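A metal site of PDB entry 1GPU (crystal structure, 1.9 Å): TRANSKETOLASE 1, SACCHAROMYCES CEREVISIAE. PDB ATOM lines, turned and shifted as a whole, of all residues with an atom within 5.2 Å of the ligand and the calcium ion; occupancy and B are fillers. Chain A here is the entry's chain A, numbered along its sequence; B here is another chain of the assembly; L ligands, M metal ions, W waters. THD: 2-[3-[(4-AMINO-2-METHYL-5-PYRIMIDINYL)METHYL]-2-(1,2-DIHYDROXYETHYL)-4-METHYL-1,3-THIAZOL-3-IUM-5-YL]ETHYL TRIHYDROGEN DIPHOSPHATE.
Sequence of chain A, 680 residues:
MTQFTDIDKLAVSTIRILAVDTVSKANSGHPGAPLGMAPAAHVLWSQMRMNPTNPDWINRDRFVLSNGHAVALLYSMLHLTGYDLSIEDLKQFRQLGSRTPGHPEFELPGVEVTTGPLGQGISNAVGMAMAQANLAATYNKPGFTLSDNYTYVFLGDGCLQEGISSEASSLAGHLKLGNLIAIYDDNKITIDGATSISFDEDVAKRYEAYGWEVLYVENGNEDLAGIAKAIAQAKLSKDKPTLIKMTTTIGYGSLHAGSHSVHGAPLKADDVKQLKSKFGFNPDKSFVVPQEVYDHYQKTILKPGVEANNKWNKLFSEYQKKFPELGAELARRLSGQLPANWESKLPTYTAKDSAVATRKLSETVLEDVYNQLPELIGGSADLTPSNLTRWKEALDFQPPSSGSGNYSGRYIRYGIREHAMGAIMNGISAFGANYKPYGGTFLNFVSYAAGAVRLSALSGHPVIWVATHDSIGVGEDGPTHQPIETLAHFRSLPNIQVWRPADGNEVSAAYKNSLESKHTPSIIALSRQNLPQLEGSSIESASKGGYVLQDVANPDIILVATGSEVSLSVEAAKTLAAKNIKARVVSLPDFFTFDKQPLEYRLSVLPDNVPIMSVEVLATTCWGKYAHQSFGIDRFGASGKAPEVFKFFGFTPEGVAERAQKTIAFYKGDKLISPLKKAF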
ATOM      1  N   HIS A  30     -32.053  25.825  -9.115  1.00  0.00           N
ATOM      2  CA  HIS A  30     -31.288  24.852  -9.886  1.00  0.00           C
ATOM      3  C   HIS A  30     -31.875  23.439  -9.876  1.00  0.00           C
ATOM      4  O   HIS A  30     -31.843  22.739  -8.859  1.00  0.00           O
ATOM      5  CB  HIS A  30     -29.864  24.821  -9.327  1.00  0.00           C
ATOM      6  CG  HIS A  30     -29.268  26.177  -9.143  1.00  0.00           C
ATOM      7  ND1 HIS A  30     -29.722  27.061  -8.187  1.00  0.00           N
ATOM      8  CD2 HIS A  30     -28.278  26.826  -9.809  1.00  0.00           C
ATOM      9  CE1 HIS A  30     -29.031  28.187  -8.265  1.00  0.00           C
ATOM     10  NE2 HIS A  30     -28.157  28.067  -9.249  1.00  0.00           N
ATOM     11  N   ALA A  33     -28.585  19.476 -10.774  1.00  0.00           N
ATOM     12  CA  ALA A  33     -27.953  18.565  -9.829  1.00  0.00           C
ATOM     13  C   ALA A  33     -28.956  17.764  -9.014  1.00  0.00           C
ATOM     14  O   ALA A  33     -28.728  16.593  -8.724  1.00  0.00           O
ATOM     15  CB  ALA A  33     -27.000  19.331  -8.919  1.00  0.00           C
ATOM     16  N   ASN A  67     -22.362  21.259  -2.870  1.00  0.00           N
ATOM     17  CA  ASN A  67     -22.866  21.934  -4.065  1.00  0.00           C
ATOM     18  C   ASN A  67     -24.234  22.455  -3.646  1.00  0.00           C
ATOM     19  O   ASN A  67     -25.285  21.957  -4.059  1.00  0.00           O
ATOM     20  CB  ASN A  67     -22.950  20.982  -5.271  1.00  0.00           C
ATOM     21  CG  ASN A  67     -23.480  19.589  -4.928  1.00  0.00           C
ATOM     22  OD1 ASN A  67     -23.789  18.806  -5.827  1.00  0.00           O
ATOM     23  ND2 ASN A  67     -23.576  19.272  -3.655  1.00  0.00           N
ATOM     24  N   HIS A  69     -26.194  24.929  -4.395  1.00  0.00           N
ATOM     25  CA  HIS A  69     -27.234  25.349  -5.323  1.00  0.00           C
ATOM     26  C   HIS A  69     -28.250  24.232  -5.560  1.00  0.00           C
ATOM     27  O   HIS A  69     -29.370  24.475  -5.999  1.00  0.00           O
ATOM     28  CB  HIS A  69     -26.630  25.795  -6.668  1.00  0.00           C
ATOM     29  CG  HIS A  69     -25.764  24.756  -7.317  1.00  0.00           C
ATOM     30  ND1 HIS A  69     -24.453  24.536  -6.944  1.00  0.00           N
ATOM     31  CD2 HIS A  69     -26.040  23.857  -8.290  1.00  0.00           C
ATOM     32  CE1 HIS A  69     -23.954  23.545  -7.668  1.00  0.00           C
ATOM     33  NE2 HIS A  69     -24.899  23.115  -8.488  1.00  0.00           N
ATOM     34  N   HIS A 103     -30.252  28.851  -0.947  1.00  0.00           N
ATOM     35  CA  HIS A 103     -29.077  28.037  -0.643  1.00  0.00           C
ATOM     36  C   HIS A 103     -29.254  27.603   0.806  1.00  0.00           C
ATOM     37  O   HIS A 103     -29.874  28.318   1.592  1.00  0.00           O
ATOM     38  CB  HIS A 103     -27.778  28.831  -0.850  1.00  0.00           C
ATOM     39  CG  HIS A 103     -27.432  29.052  -2.288  1.00  0.00           C
ATOM     40  ND1 HIS A 103     -27.887  30.142  -3.008  1.00  0.00           N
ATOM     41  CD2 HIS A 103     -26.753  28.291  -3.171  1.00  0.00           C
ATOM     42  CE1 HIS A 103     -27.517  30.029  -4.267  1.00  0.00           C
ATOM     43  NE2 HIS A 103     -26.830  28.913  -4.393  1.00  0.00           N
ATOM     44  N   GLY A 116     -23.227  27.251  -0.512  1.00  0.00           N
ATOM     45  CA  GLY A 116     -23.641  28.130  -1.596  1.00  0.00           C
ATOM     46  C   GLY A 116     -22.325  28.586  -2.170  1.00  0.00           C
ATOM     47  O   GLY A 116     -22.120  28.570  -3.384  1.00  0.00           O
ATOM     48  N   PRO A 117     -21.402  29.055  -1.305  1.00  0.00           N
ATOM     49  CA  PRO A 117     -20.092  29.488  -1.799  1.00  0.00           C
ATOM     50  C   PRO A 117     -19.352  28.163  -1.989  1.00  0.00           C
ATOM     51  O   PRO A 117     -19.096  27.440  -1.021  1.00  0.00           O
ATOM     52  CB  PRO A 117     -19.535  30.314  -0.633  1.00  0.00           C
ATOM     53  CG  PRO A 117     -20.765  30.863   0.023  1.00  0.00           C
ATOM     54  CD  PRO A 117     -21.672  29.643   0.024  1.00  0.00           C
ATOM     55  N   LEU A 118     -19.042  27.837  -3.243  1.00  0.00           N
ATOM     56  CA  LEU A 118     -18.380  26.573  -3.561  1.00  0.00           C
ATOM     57  C   LEU A 118     -17.085  26.278  -2.806  1.00  0.00           C
ATOM     58  O   LEU A 118     -16.293  27.165  -2.535  1.00  0.00           O
ATOM     59  CB  LEU A 118     -18.131  26.499  -5.075  1.00  0.00           C
ATOM     60  CG  LEU A 118     -19.422  26.524  -5.903  1.00  0.00           C
ATOM     61  CD1 LEU A 118     -19.080  26.806  -7.358  1.00  0.00           C
ATOM     62  CD2 LEU A 118     -20.137  25.192  -5.773  1.00  0.00           C
ATOM     63  N   GLY A 156     -19.699  18.859  -6.312  1.00  0.00           N
ATOM     64  CA  GLY A 156     -19.603  18.823  -7.769  1.00  0.00           C
ATOM     65  C   GLY A 156     -18.276  19.355  -8.274  1.00  0.00           C
ATOM     66  O   GLY A 156     -17.339  19.558  -7.505  1.00  0.00           O
ATOM     67  N   ASP A 157     -18.204  19.583  -9.584  1.00  0.00           N
ATOM     68  CA  ASP A 157     -16.972  20.087 -10.201  1.00  0.00           C
ATOM     69  C   ASP A 157     -16.578  21.450  -9.642  1.00  0.00           C
ATOM     70  O   ASP A 157     -15.391  21.746  -9.523  1.00  0.00           O
ATOM     71  CB  ASP A 157     -17.161  20.180 -11.708  1.00  0.00           C
ATOM     72  CG  ASP A 157     -17.450  18.831 -12.337  1.00  0.00           C
ATOM     73  OD1 ASP A 157     -16.571  17.955 -12.315  1.00  0.00           O
ATOM     74  OD2 ASP A 157     -18.560  18.644 -12.854  1.00  0.00           O
ATOM     75  N   GLY A 158     -17.564  22.256  -9.303  1.00  0.00           N
ATOM     76  CA  GLY A 158     -17.308  23.588  -8.775  1.00  0.00           C
ATOM     77  C   GLY A 158     -16.505  23.551  -7.492  1.00  0.00           C
ATOM     78  O   GLY A 158     -15.536  24.296  -7.336  1.00  0.00           O
ATOM     79  N   CYS A 159     -16.905  22.684  -6.556  1.00  0.00           N
ATOM     80  CA  CYS A 159     -16.192  22.578  -5.298  1.00  0.00           C
ATOM     81  C   CYS A 159     -14.789  22.041  -5.507  1.00  0.00           C
ATOM     82  O   CYS A 159     -13.833  22.459  -4.837  1.00  0.00           O
ATOM     83  CB  CYS A 159     -16.966  21.673  -4.323  1.00  0.00           C
ATOM     84  SG  CYS A 159     -18.558  22.385  -3.759  1.00  0.00           S
ATOM     85  N   GLU A 162     -12.343  24.942  -6.602  1.00  0.00           N
ATOM     86  CA  GLU A 162     -11.974  25.975  -5.625  1.00  0.00           C
ATOM     87  C   GLU A 162     -10.795  25.505  -4.792  1.00  0.00           C
ATOM     88  O   GLU A 162     -10.836  24.421  -4.194  1.00  0.00           O
ATOM     89  CB  GLU A 162     -13.158  26.282  -4.707  1.00  0.00           C
ATOM     90  CG  GLU A 162     -14.245  27.132  -5.346  1.00  0.00           C
ATOM     91  CD  GLU A 162     -13.814  28.574  -5.569  1.00  0.00           C
ATOM     92  OE1 GLU A 162     -12.679  28.930  -5.188  1.00  0.00           O
ATOM     93  OE2 GLU A 162     -14.619  29.347  -6.109  1.00  0.00           O
ATOM     94  N   ASP A 185     -20.384  14.385  -7.818  1.00  0.00           N
ATOM     95  CA  ASP A 185     -21.340  14.371  -8.924  1.00  0.00           C
ATOM     96  C   ASP A 185     -20.574  14.659 -10.216  1.00  0.00           C
ATOM     97  O   ASP A 185     -20.428  15.806 -10.629  1.00  0.00           O
ATOM     98  CB  ASP A 185     -22.441  15.406  -8.691  1.00  0.00           C
ATOM     99  CG  ASP A 185     -23.548  15.327  -9.720  1.00  0.00           C
ATOM    100  OD1 ASP A 185     -23.673  14.265 -10.367  1.00  0.00           O
ATOM    101  OD2 ASP A 185     -24.308  16.311  -9.881  1.00  0.00           O
ATOM    102  N   ASN A 187     -20.750  14.964 -13.555  1.00  0.00           N
ATOM    103  CA  ASN A 187     -21.663  15.151 -14.687  1.00  0.00           C
ATOM    104  C   ASN A 187     -21.100  15.958 -15.867  1.00  0.00           C
ATOM    105  O   ASN A 187     -21.822  16.280 -16.814  1.00  0.00           O
ATOM    106  CB  ASN A 187     -22.985  15.792 -14.202  1.00  0.00           C
ATOM    107  CG  ASN A 187     -22.776  17.172 -13.645  1.00  0.00           C
ATOM    108  OD1 ASN A 187     -21.800  17.825 -13.984  1.00  0.00           O
ATOM    109  ND2 ASN A 187     -23.706  17.633 -12.823  1.00  0.00           N
ATOM    110  N   LYS A 188     -19.810  16.276 -15.794  1.00  0.00           N
ATOM    111  CA  LYS A 188     -19.095  16.989 -16.856  1.00  0.00           C
ATOM    112  C   LYS A 188     -19.689  18.296 -17.387  1.00  0.00           C
ATOM    113  O   LYS A 188     -19.497  18.658 -18.554  1.00  0.00           O
ATOM    114  CB  LYS A 188     -18.832  16.010 -18.002  1.00  0.00           C
ATOM    115  CG  LYS A 188     -17.873  14.912 -17.541  1.00  0.00           C
ATOM    116  CD  LYS A 188     -17.842  13.712 -18.431  1.00  0.00           C
ATOM    117  CE  LYS A 188     -16.835  12.694 -17.917  1.00  0.00           C
ATOM    118  NZ  LYS A 188     -17.136  12.210 -16.539  1.00  0.00           N
ATOM    119  N   ILE A 189     -20.354  19.032 -16.502  1.00  0.00           N
ATOM    120  CA  ILE A 189     -20.978  20.292 -16.858  1.00  0.00           C
ATOM    121  C   ILE A 189     -20.817  21.346 -15.758  1.00  0.00           C
ATOM    122  O   ILE A 189     -20.930  21.029 -14.587  1.00  0.00           O
ATOM    123  CB  ILE A 189     -22.496  20.120 -17.094  1.00  0.00           C
ATOM    124  CG1 ILE A 189     -22.756  19.410 -18.432  1.00  0.00           C
ATOM    125  CG2 ILE A 189     -23.198  21.475 -17.037  1.00  0.00           C
ATOM    126  CD1 ILE A 189     -22.486  20.277 -19.655  1.00  0.00           C
ATOM    127  N   THR A 190     -20.548  22.589 -16.128  1.00  0.00           N
ATOM    128  CA  THR A 190     -20.492  23.673 -15.169  1.00  0.00           C
ATOM    129  C   THR A 190     -21.207  24.819 -15.873  1.00  0.00           C
ATOM    130  O   THR A 190     -21.719  24.633 -16.978  1.00  0.00           O
ATOM    131  CB  THR A 190     -19.043  24.093 -14.772  1.00  0.00           C
ATOM    132  OG1 THR A 190     -18.291  24.462 -15.940  1.00  0.00           O
ATOM    133  CG2 THR A 190     -18.345  22.945 -14.053  1.00  0.00           C
ATOM    134  N   ILE A 191     -21.277  25.989 -15.250  1.00  0.00           N
ATOM    135  CA  ILE A 191     -21.987  27.104 -15.860  1.00  0.00           C
ATOM    136  C   ILE A 191     -21.531  27.503 -17.267  1.00  0.00           C
ATOM    137  O   ILE A 191     -22.356  27.806 -18.121  1.00  0.00           O
ATOM    138  CB  ILE A 191     -21.961  28.339 -14.924  1.00  0.00           C
ATOM    139  CG1 ILE A 191     -22.864  28.058 -13.714  1.00  0.00           C
ATOM    140  CG2 ILE A 191     -22.425  29.585 -15.669  1.00  0.00           C
ATOM    141  CD1 ILE A 191     -22.947  29.219 -12.730  1.00  0.00           C
ATOM    142  N   THR A 195     -17.062  20.640 -18.882  1.00  0.00           N
ATOM    143  CA  THR A 195     -15.917  20.813 -17.989  1.00  0.00           C
ATOM    144  C   THR A 195     -14.604  20.832 -18.768  1.00  0.00           C
ATOM    145  O   THR A 195     -13.653  21.477 -18.349  1.00  0.00           O
ATOM    146  CB  THR A 195     -15.837  19.679 -16.938  1.00  0.00           C
ATOM    147  OG1 THR A 195     -15.986  18.408 -17.580  1.00  0.00           O
ATOM    148  CG2 THR A 195     -16.917  19.858 -15.883  1.00  0.00           C
ATOM    149  N   ILE A 250     -26.539  15.487 -15.732  1.00  0.00           N
ATOM    150  CA  ILE A 250     -27.180  16.637 -15.091  1.00  0.00           C
ATOM    151  C   ILE A 250     -28.594  16.778 -15.661  1.00  0.00           C
ATOM    152  O   ILE A 250     -28.808  16.664 -16.864  1.00  0.00           O
ATOM    153  CB  ILE A 250     -26.368  17.943 -15.323  1.00  0.00           C
ATOM    154  CG1 ILE A 250     -26.922  19.059 -14.440  1.00  0.00           C
ATOM    155  CG2 ILE A 250     -26.431  18.354 -16.797  1.00  0.00           C
ATOM    156  CD1 ILE A 250     -26.119  20.347 -14.499  1.00  0.00           C
ATOM    157  N   HIS A 263     -28.583  23.666 -15.533  1.00  0.00           N
ATOM    158  CA  HIS A 263     -27.848  23.896 -14.299  1.00  0.00           C
ATOM    159  C   HIS A 263     -28.587  24.800 -13.316  1.00  0.00           C
ATOM    160  O   HIS A 263     -28.784  24.435 -12.162  1.00  0.00           O
ATOM    161  CB  HIS A 263     -26.477  24.525 -14.559  1.00  0.00           C
ATOM    162  CG  HIS A 263     -25.942  25.298 -13.393  1.00  0.00           C
ATOM    163  ND1 HIS A 263     -25.307  24.689 -12.331  1.00  0.00           N
ATOM    164  CD2 HIS A 263     -26.052  26.605 -13.076  1.00  0.00           C
ATOM    165  CE1 HIS A 263     -25.038  25.598 -11.405  1.00  0.00           C
ATOM    166  NE2 HIS A 263     -25.478  26.770 -11.832  1.00  0.00           N
ATOM    167  N   ALA B 381     -14.821  33.474 -14.226  1.00  0.00           N
ATOM    168  CA  ALA B 381     -14.597  32.311 -13.379  1.00  0.00           C
ATOM    169  C   ALA B 381     -15.872  31.465 -13.434  1.00  0.00           C
ATOM    170  O   ALA B 381     -16.635  31.418 -12.478  1.00  0.00           O
ATOM    171  CB  ALA B 381     -14.305  32.743 -11.951  1.00  0.00           C
ATOM    172  N   ASP B 382     -16.093  30.822 -14.587  1.00  0.00           N
ATOM    173  CA  ASP B 382     -17.258  29.970 -14.816  1.00  0.00           C
ATOM    174  C   ASP B 382     -18.600  30.699 -14.701  1.00  0.00           C
ATOM    175  O   ASP B 382     -19.597  30.097 -14.282  1.00  0.00           O
ATOM    176  CB  ASP B 382     -17.238  28.763 -13.878  1.00  0.00           C
ATOM    177  CG  ASP B 382     -18.154  27.638 -14.356  1.00  0.00           C
ATOM    178  OD1 ASP B 382     -18.040  27.224 -15.524  1.00  0.00           O
ATOM    179  OD2 ASP B 382     -18.987  27.168 -13.551  1.00  0.00           O
ATOM    180  N   LEU B 383     -18.630  31.979 -15.052  1.00  0.00           N
ATOM    181  CA  LEU B 383     -19.863  32.767 -14.980  1.00  0.00           C
ATOM    182  C   LEU B 383     -20.043  33.638 -16.217  1.00  0.00           C
ATOM    183  O   LEU B 383     -20.599  34.735 -16.144  1.00  0.00           O
ATOM    184  CB  LEU B 383     -19.874  33.643 -13.724  1.00  0.00           C
ATOM    185  CG  LEU B 383     -20.080  32.927 -12.373  1.00  0.00           C
ATOM    186  CD1 LEU B 383     -19.961  33.934 -11.236  1.00  0.00           C
ATOM    187  CD2 LEU B 383     -21.452  32.242 -12.356  1.00  0.00           C
ATOM    188  N   ILE B 416     -14.041  27.666 -11.883  1.00  0.00           N
ATOM    189  CA  ILE B 416     -14.402  28.218 -10.570  1.00  0.00           C
ATOM    190  C   ILE B 416     -13.121  28.407  -9.759  1.00  0.00           C
ATOM    191  O   ILE B 416     -12.851  27.684  -8.789  1.00  0.00           O
ATOM    192  CB  ILE B 416     -15.374  27.268  -9.819  1.00  0.00           C
ATOM    193  CG1 ILE B 416     -16.595  26.956 -10.689  1.00  0.00           C
ATOM    194  CG2 ILE B 416     -15.857  27.945  -8.541  1.00  0.00           C
ATOM    195  CD1 ILE B 416     -16.352  25.951 -11.804  1.00  0.00           C
ATOM    196  N   GLU B 418     -11.535  31.881  -8.567  1.00  0.00           N
ATOM    197  CA  GLU B 418     -11.390  33.330  -8.429  1.00  0.00           C
ATOM    198  C   GLU B 418      -9.995  33.778  -8.011  1.00  0.00           C
ATOM    199  O   GLU B 418      -9.417  34.678  -8.609  1.00  0.00           O
ATOM    200  CB  GLU B 418     -12.394  33.891  -7.417  1.00  0.00           C
ATOM    201  CG  GLU B 418     -13.856  33.702  -7.773  1.00  0.00           C
ATOM    202  CD  GLU B 418     -14.392  32.351  -7.354  1.00  0.00           C
ATOM    203  OE1 GLU B 418     -13.695  31.636  -6.608  1.00  0.00           O
ATOM    204  OE2 GLU B 418     -15.522  32.004  -7.763  1.00  0.00           O
ATOM    205  N   THR B 441     -16.799  37.715 -12.279  1.00  0.00           N
ATOM    206  CA  THR B 441     -17.325  36.839 -11.236  1.00  0.00           C
ATOM    207  C   THR B 441     -18.323  37.665 -10.459  1.00  0.00           C
ATOM    208  O   THR B 441     -18.469  38.860 -10.716  1.00  0.00           O
ATOM    209  CB  THR B 441     -16.235  36.319 -10.267  1.00  0.00           C
ATOM    210  OG1 THR B 441     -16.812  35.348  -9.390  1.00  0.00           O
ATOM    211  CG2 THR B 441     -15.663  37.451  -9.422  1.00  0.00           C
ATOM    212  N   PHE B 442     -19.030  37.047  -9.520  1.00  0.00           N
ATOM    213  CA  PHE B 442     -19.983  37.778  -8.710  1.00  0.00           C
ATOM    214  C   PHE B 442     -19.184  38.601  -7.701  1.00  0.00           C
ATOM    215  O   PHE B 442     -18.191  38.114  -7.159  1.00  0.00           O
ATOM    216  CB  PHE B 442     -20.934  36.840  -7.955  1.00  0.00           C
ATOM    217  CG  PHE B 442     -21.846  36.034  -8.854  1.00  0.00           C
ATOM    218  CD1 PHE B 442     -22.338  36.577 -10.040  1.00  0.00           C
ATOM    219  CD2 PHE B 442     -22.236  34.754  -8.488  1.00  0.00           C
ATOM    220  CE1 PHE B 442     -23.215  35.845 -10.848  1.00  0.00           C
ATOM    221  CE2 PHE B 442     -23.114  34.005  -9.291  1.00  0.00           C
ATOM    222  CZ  PHE B 442     -23.607  34.557 -10.471  1.00  0.00           C
ATOM    223  N   PHE B 445     -17.886  37.031  -4.553  1.00  0.00           N
ATOM    224  CA  PHE B 445     -16.818  36.047  -4.591  1.00  0.00           C
ATOM    225  C   PHE B 445     -15.464  36.599  -5.002  1.00  0.00           C
ATOM    226  O   PHE B 445     -14.467  35.881  -5.072  1.00  0.00           O
ATOM    227  CB  PHE B 445     -17.268  34.845  -5.441  1.00  0.00           C
ATOM    228  CG  PHE B 445     -18.503  34.165  -4.891  1.00  0.00           C
ATOM    229  CD1 PHE B 445     -18.577  33.841  -3.537  1.00  0.00           C
ATOM    230  CD2 PHE B 445     -19.600  33.894  -5.696  1.00  0.00           C
ATOM    231  CE1 PHE B 445     -19.732  33.262  -2.992  1.00  0.00           C
ATOM    232  CE2 PHE B 445     -20.760  33.312  -5.164  1.00  0.00           C
ATOM    233  CZ  PHE B 445     -20.826  33.000  -3.809  1.00  0.00           C
ATOM    234  N   TYR B 448     -13.003  35.917  -2.475  1.00  0.00           N
ATOM    235  CA  TYR B 448     -12.262  34.653  -2.462  1.00  0.00           C
ATOM    236  C   TYR B 448     -10.845  34.902  -2.962  1.00  0.00           C
ATOM    237  O   TYR B 448      -9.932  34.099  -2.715  1.00  0.00           O
ATOM    238  CB  TYR B 448     -12.911  33.627  -3.394  1.00  0.00           C
ATOM    239  CG  TYR B 448     -13.789  32.578  -2.730  1.00  0.00           C
ATOM    240  CD1 TYR B 448     -14.874  32.933  -1.927  1.00  0.00           C
ATOM    241  CD2 TYR B 448     -13.553  31.217  -2.956  1.00  0.00           C
ATOM    242  CE1 TYR B 448     -15.710  31.950  -1.376  1.00  0.00           C
ATOM    243  CE2 TYR B 448     -14.381  30.238  -2.410  1.00  0.00           C
ATOM    244  CZ  TYR B 448     -15.461  30.611  -1.629  1.00  0.00           C
ATOM    245  OH  TYR B 448     -16.309  29.634  -1.139  1.00  0.00           O
ATOM    246  N   ASP B 477     -30.996  33.976  -4.798  1.00  0.00           N
ATOM    247  CA  ASP B 477     -29.830  33.222  -4.359  1.00  0.00           C
ATOM    248  C   ASP B 477     -29.548  33.440  -2.882  1.00  0.00           C
ATOM    249  O   ASP B 477     -28.914  32.602  -2.234  1.00  0.00           O
ATOM    250  CB  ASP B 477     -28.607  33.559  -5.223  1.00  0.00           C
ATOM    251  CG  ASP B 477     -28.601  32.783  -6.530  1.00  0.00           C
ATOM    252  OD1 ASP B 477     -29.367  31.807  -6.629  1.00  0.00           O
ATOM    253  OD2 ASP B 477     -27.843  33.139  -7.446  1.00  0.00           O
ATOM    254  N   HIS B 481     -24.856  34.982  -1.354  1.00  0.00           N
ATOM    255  CA  HIS B 481     -24.503  35.573  -2.649  1.00  0.00           C
ATOM    256  C   HIS B 481     -24.650  37.082  -2.689  1.00  0.00           C
ATOM    257  O   HIS B 481     -24.312  37.716  -3.691  1.00  0.00           O
ATOM    258  CB  HIS B 481     -25.370  34.983  -3.761  1.00  0.00           C
ATOM    259  CG  HIS B 481     -24.963  33.601  -4.181  1.00  0.00           C
ATOM    260  ND1 HIS B 481     -24.848  32.550  -3.285  1.00  0.00           N
ATOM    261  CD2 HIS B 481     -24.648  33.094  -5.394  1.00  0.00           C
ATOM    262  CE1 HIS B 481     -24.484  31.462  -3.936  1.00  0.00           C
ATOM    263  NE2 HIS B 481     -24.359  31.763  -5.217  1.00  0.00           N
HETATM  264  N1' THD L   1     -17.751  31.133  -6.754  1.00  0.00           N
HETATM  265  C2' THD L   1     -18.051  30.614  -5.547  1.00  0.00           C
HETATM  266  CM2 THD L   1     -17.023  30.591  -4.530  1.00  0.00           C
HETATM  267  N3' THD L   1     -19.260  30.133  -5.307  1.00  0.00           N
HETATM  268  C4' THD L   1     -20.258  30.159  -6.290  1.00  0.00           C
HETATM  269  N4' THD L   1     -21.427  29.652  -5.909  1.00  0.00           N
HETATM  270  C5' THD L   1     -19.993  30.715  -7.619  1.00  0.00           C
HETATM  271  C6' THD L   1     -18.700  31.176  -7.769  1.00  0.00           C
HETATM  272  C7' THD L   1     -21.004  30.796  -8.778  1.00  0.00           C
HETATM  273  N3  THD L   1     -21.551  29.370  -9.079  1.00  0.00           N
HETATM  274  C2  THD L   1     -22.731  28.774  -8.597  1.00  0.00           C
HETATM  275  S1  THD L   1     -22.865  27.152  -9.138  1.00  0.00           S
HETATM  276  C5  THD L   1     -21.419  27.272 -10.013  1.00  0.00           C
HETATM  277  C4  THD L   1     -20.860  28.516  -9.869  1.00  0.00           C
HETATM  278  CM4 THD L   1     -19.581  28.923 -10.516  1.00  0.00           C
HETATM  279  C6  THD L   1     -20.870  26.117 -10.828  1.00  0.00           C
HETATM  280  C7  THD L   1     -21.777  24.961 -10.994  1.00  0.00           C
HETATM  281  O7  THD L   1     -20.923  23.850 -11.250  1.00  0.00           O
HETATM  282  PA  THD L   1     -21.041  22.637 -10.295  1.00  0.00           P
HETATM  283  O1A THD L   1     -20.554  22.829  -8.883  1.00  0.00           O
HETATM  284  O2A THD L   1     -20.331  21.711 -11.120  1.00  0.00           O
HETATM  285  O3A THD L   1     -22.503  21.980 -10.463  1.00  0.00           O
HETATM  286  PB  THD L   1     -23.682  21.608 -11.498  1.00  0.00           P
HETATM  287  O1B THD L   1     -23.186  20.283 -11.813  1.00  0.00           O
HETATM  288  O2B THD L   1     -24.899  21.547 -10.699  1.00  0.00           O
HETATM  289  O3B THD L   1     -23.754  22.640 -12.563  1.00  0.00           O
HETATM  290  C8  THD L   1     -23.530  29.540  -7.975  1.00  0.00           C
HETATM  291  O9  THD L   1     -23.495  30.764  -7.707  1.00  0.00           O
HETATM  292  C9  THD L   1     -24.658  28.742  -7.551  1.00  0.00           C
HETATM  293  O10 THD L   1     -24.683  28.652  -6.134  1.00  0.00           O
HETATM  294 CA    CA M   1     -20.836  19.697 -12.638  1.00  0.00          CA
HETATM  295  O   HOH W   1     -16.913  32.623 -10.048  1.00  0.00           O
HETATM  296  O   HOH W   2     -27.600  22.213 -10.905  1.00  0.00           O
HETATM  297  O   HOH W   3     -19.675  21.665  -6.527  1.00  0.00           O
HETATM  298  O   HOH W   4     -20.930  18.226 -10.316  1.00  0.00           O
HETATM  299  O   HOH W   5     -23.439  18.733  -8.912  1.00  0.00           O
HETATM  300  O   HOH W   6     -23.377  26.187  -5.053  1.00  0.00           O
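Along chain A the residues within 4 Å of the calcium ion span positions 157 to 189.
The nearest printed residue that does not touch the calcium ion is Thr 190 (4.3 Å).
Water W4 bridges O of Asp 185 (2.5 Å) and N of Asp 157 (3.1 Å).
Water W3 lies within hydrogen-bond range of an oxygen (O1A) of the ligand, the backbone NH (N) of Gly 156 and the backbone NH (N) of Cys 159.
Water W2 lies within hydrogen-bond range of O2B of the ligand, O of His 263 and N of Ala 33.
Water W6 lies within hydrogen-bond range of ND1 of His 69, O10 of the ligand and O of Gly 116.
Water W1 lies within hydrogen-bond range of O of Ala 381 of chain B (2.7 Å), OE2 of Glu 418 of chain B (2.7 Å) and OG1 of Thr 441 of chain B (2.8 Å).
Water W5 lies within hydrogen-bond range of OD2 of Asp 185 and OD1 of Asn 67.
O of Leu 118 is in hydrogen-bond range of OH of Tyr 448 of chain B, 2.8 Å away.
ND2 of Asn 187 sits at hydrogen-bond distance from OD2 of Asp 185, at 3.3 Å.
A ring nitrogen (ND1) of His 103 lies within hydrogen-bond range of the backbone carbonyl oxygen (O) of Asp 477 of chain B, 2.8 Å away.
OE1 of Glu 418 of chain B sits close to OE2 of Glu 162, 2.5 Å away.
The backbone carbonyl oxygen (O) of His 69 sits close to a ring nitrogen (ND1) of His 30.
OD1 of Asp 382 of chain B sits at hydrogen-bond distance from OG1 of Thr 190, 2.8 Å away.
OD2 of Asp 382 of chain B is in hydrogen-bond range of N of Ile 191 (3.1 Å).
A ring nitrogen (NE2) of His 69 is in hydrogen-bond range of an oxygen (O2B) of the ligand, 2.7 Å away.
An oxygen (O2A) of the ligand lies close to the backbone NH of Asp 157.
The side-chain carboxylate (OE2) of Glu 418 of chain B is in hydrogen-bond range of a nitrogen (N1') of the ligand (2.6 Å).
A ring nitrogen (NE2) of His 103 sits at hydrogen-bond distance from an oxygen (O10) of the ligand (2.8 Å).
N of Leu 118 lies within hydrogen-bond range of N3' of the ligand.
N of Gly 158 lies within hydrogen-bond range of O1A of the ligand, at 3.1 Å.
An oxygen (O3B) of the ligand lies within hydrogen-bond range of a ring nitrogen (ND1) of His 263 (2.6 Å).
O of Gly 116 is in hydrogen-bond range of N4' of the ligand, 2.8 Å away.
NE2 of His 481 of chain B is in hydrogen-bond range of O9 of the ligand (2.8 Å).
Residues that only touch the ligand: Glu 162 (3.1 Å), Tyr 448 of chain B (3.3 Å), Phe 445 of chain B (3.4 Å), Asp 382 of chain B (3.5 Å), Ala 33 (3.5 Å), Ile 416 of chain B (3.6 Å), Ile 191 (3.6 Å), Phe 442 of chain B (3.6 Å), Pro 117 (3.7 Å), Thr 190 (3.8 Å), Ile 250 (3.8 Å), Leu 383 of chain B (3.9 Å) and His 30 (3.9 Å).
Hydrophobic or aromatic side chains that line the ligand: Ala 33, His 69, His 103, Leu 118, Ile 191, Ile 250, His 263, Leu 383 of chain B, Ile 416 of chain B, Phe 442 of chain B, Phe 445 of chain B, Tyr 448 of chain B and His 481 of chain B.
Of the 33 residues printed, 24 come within 4 Å of the ligand.
The nearest printed residue that does not touch the ligand is Gly 156 (4.2 Å).
The calcium ion is bound by O of Ile 189 (2.4 Å), OD1 of Asn 187 (2.5 Å), OD2 of Asp 157 (2.5 Å), O1B of the ligand (2.6 Å), O2A of the ligand (2.6 Å) and water W4 (2.8 Å).
The calcium ion has six donor atoms within binding distance.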
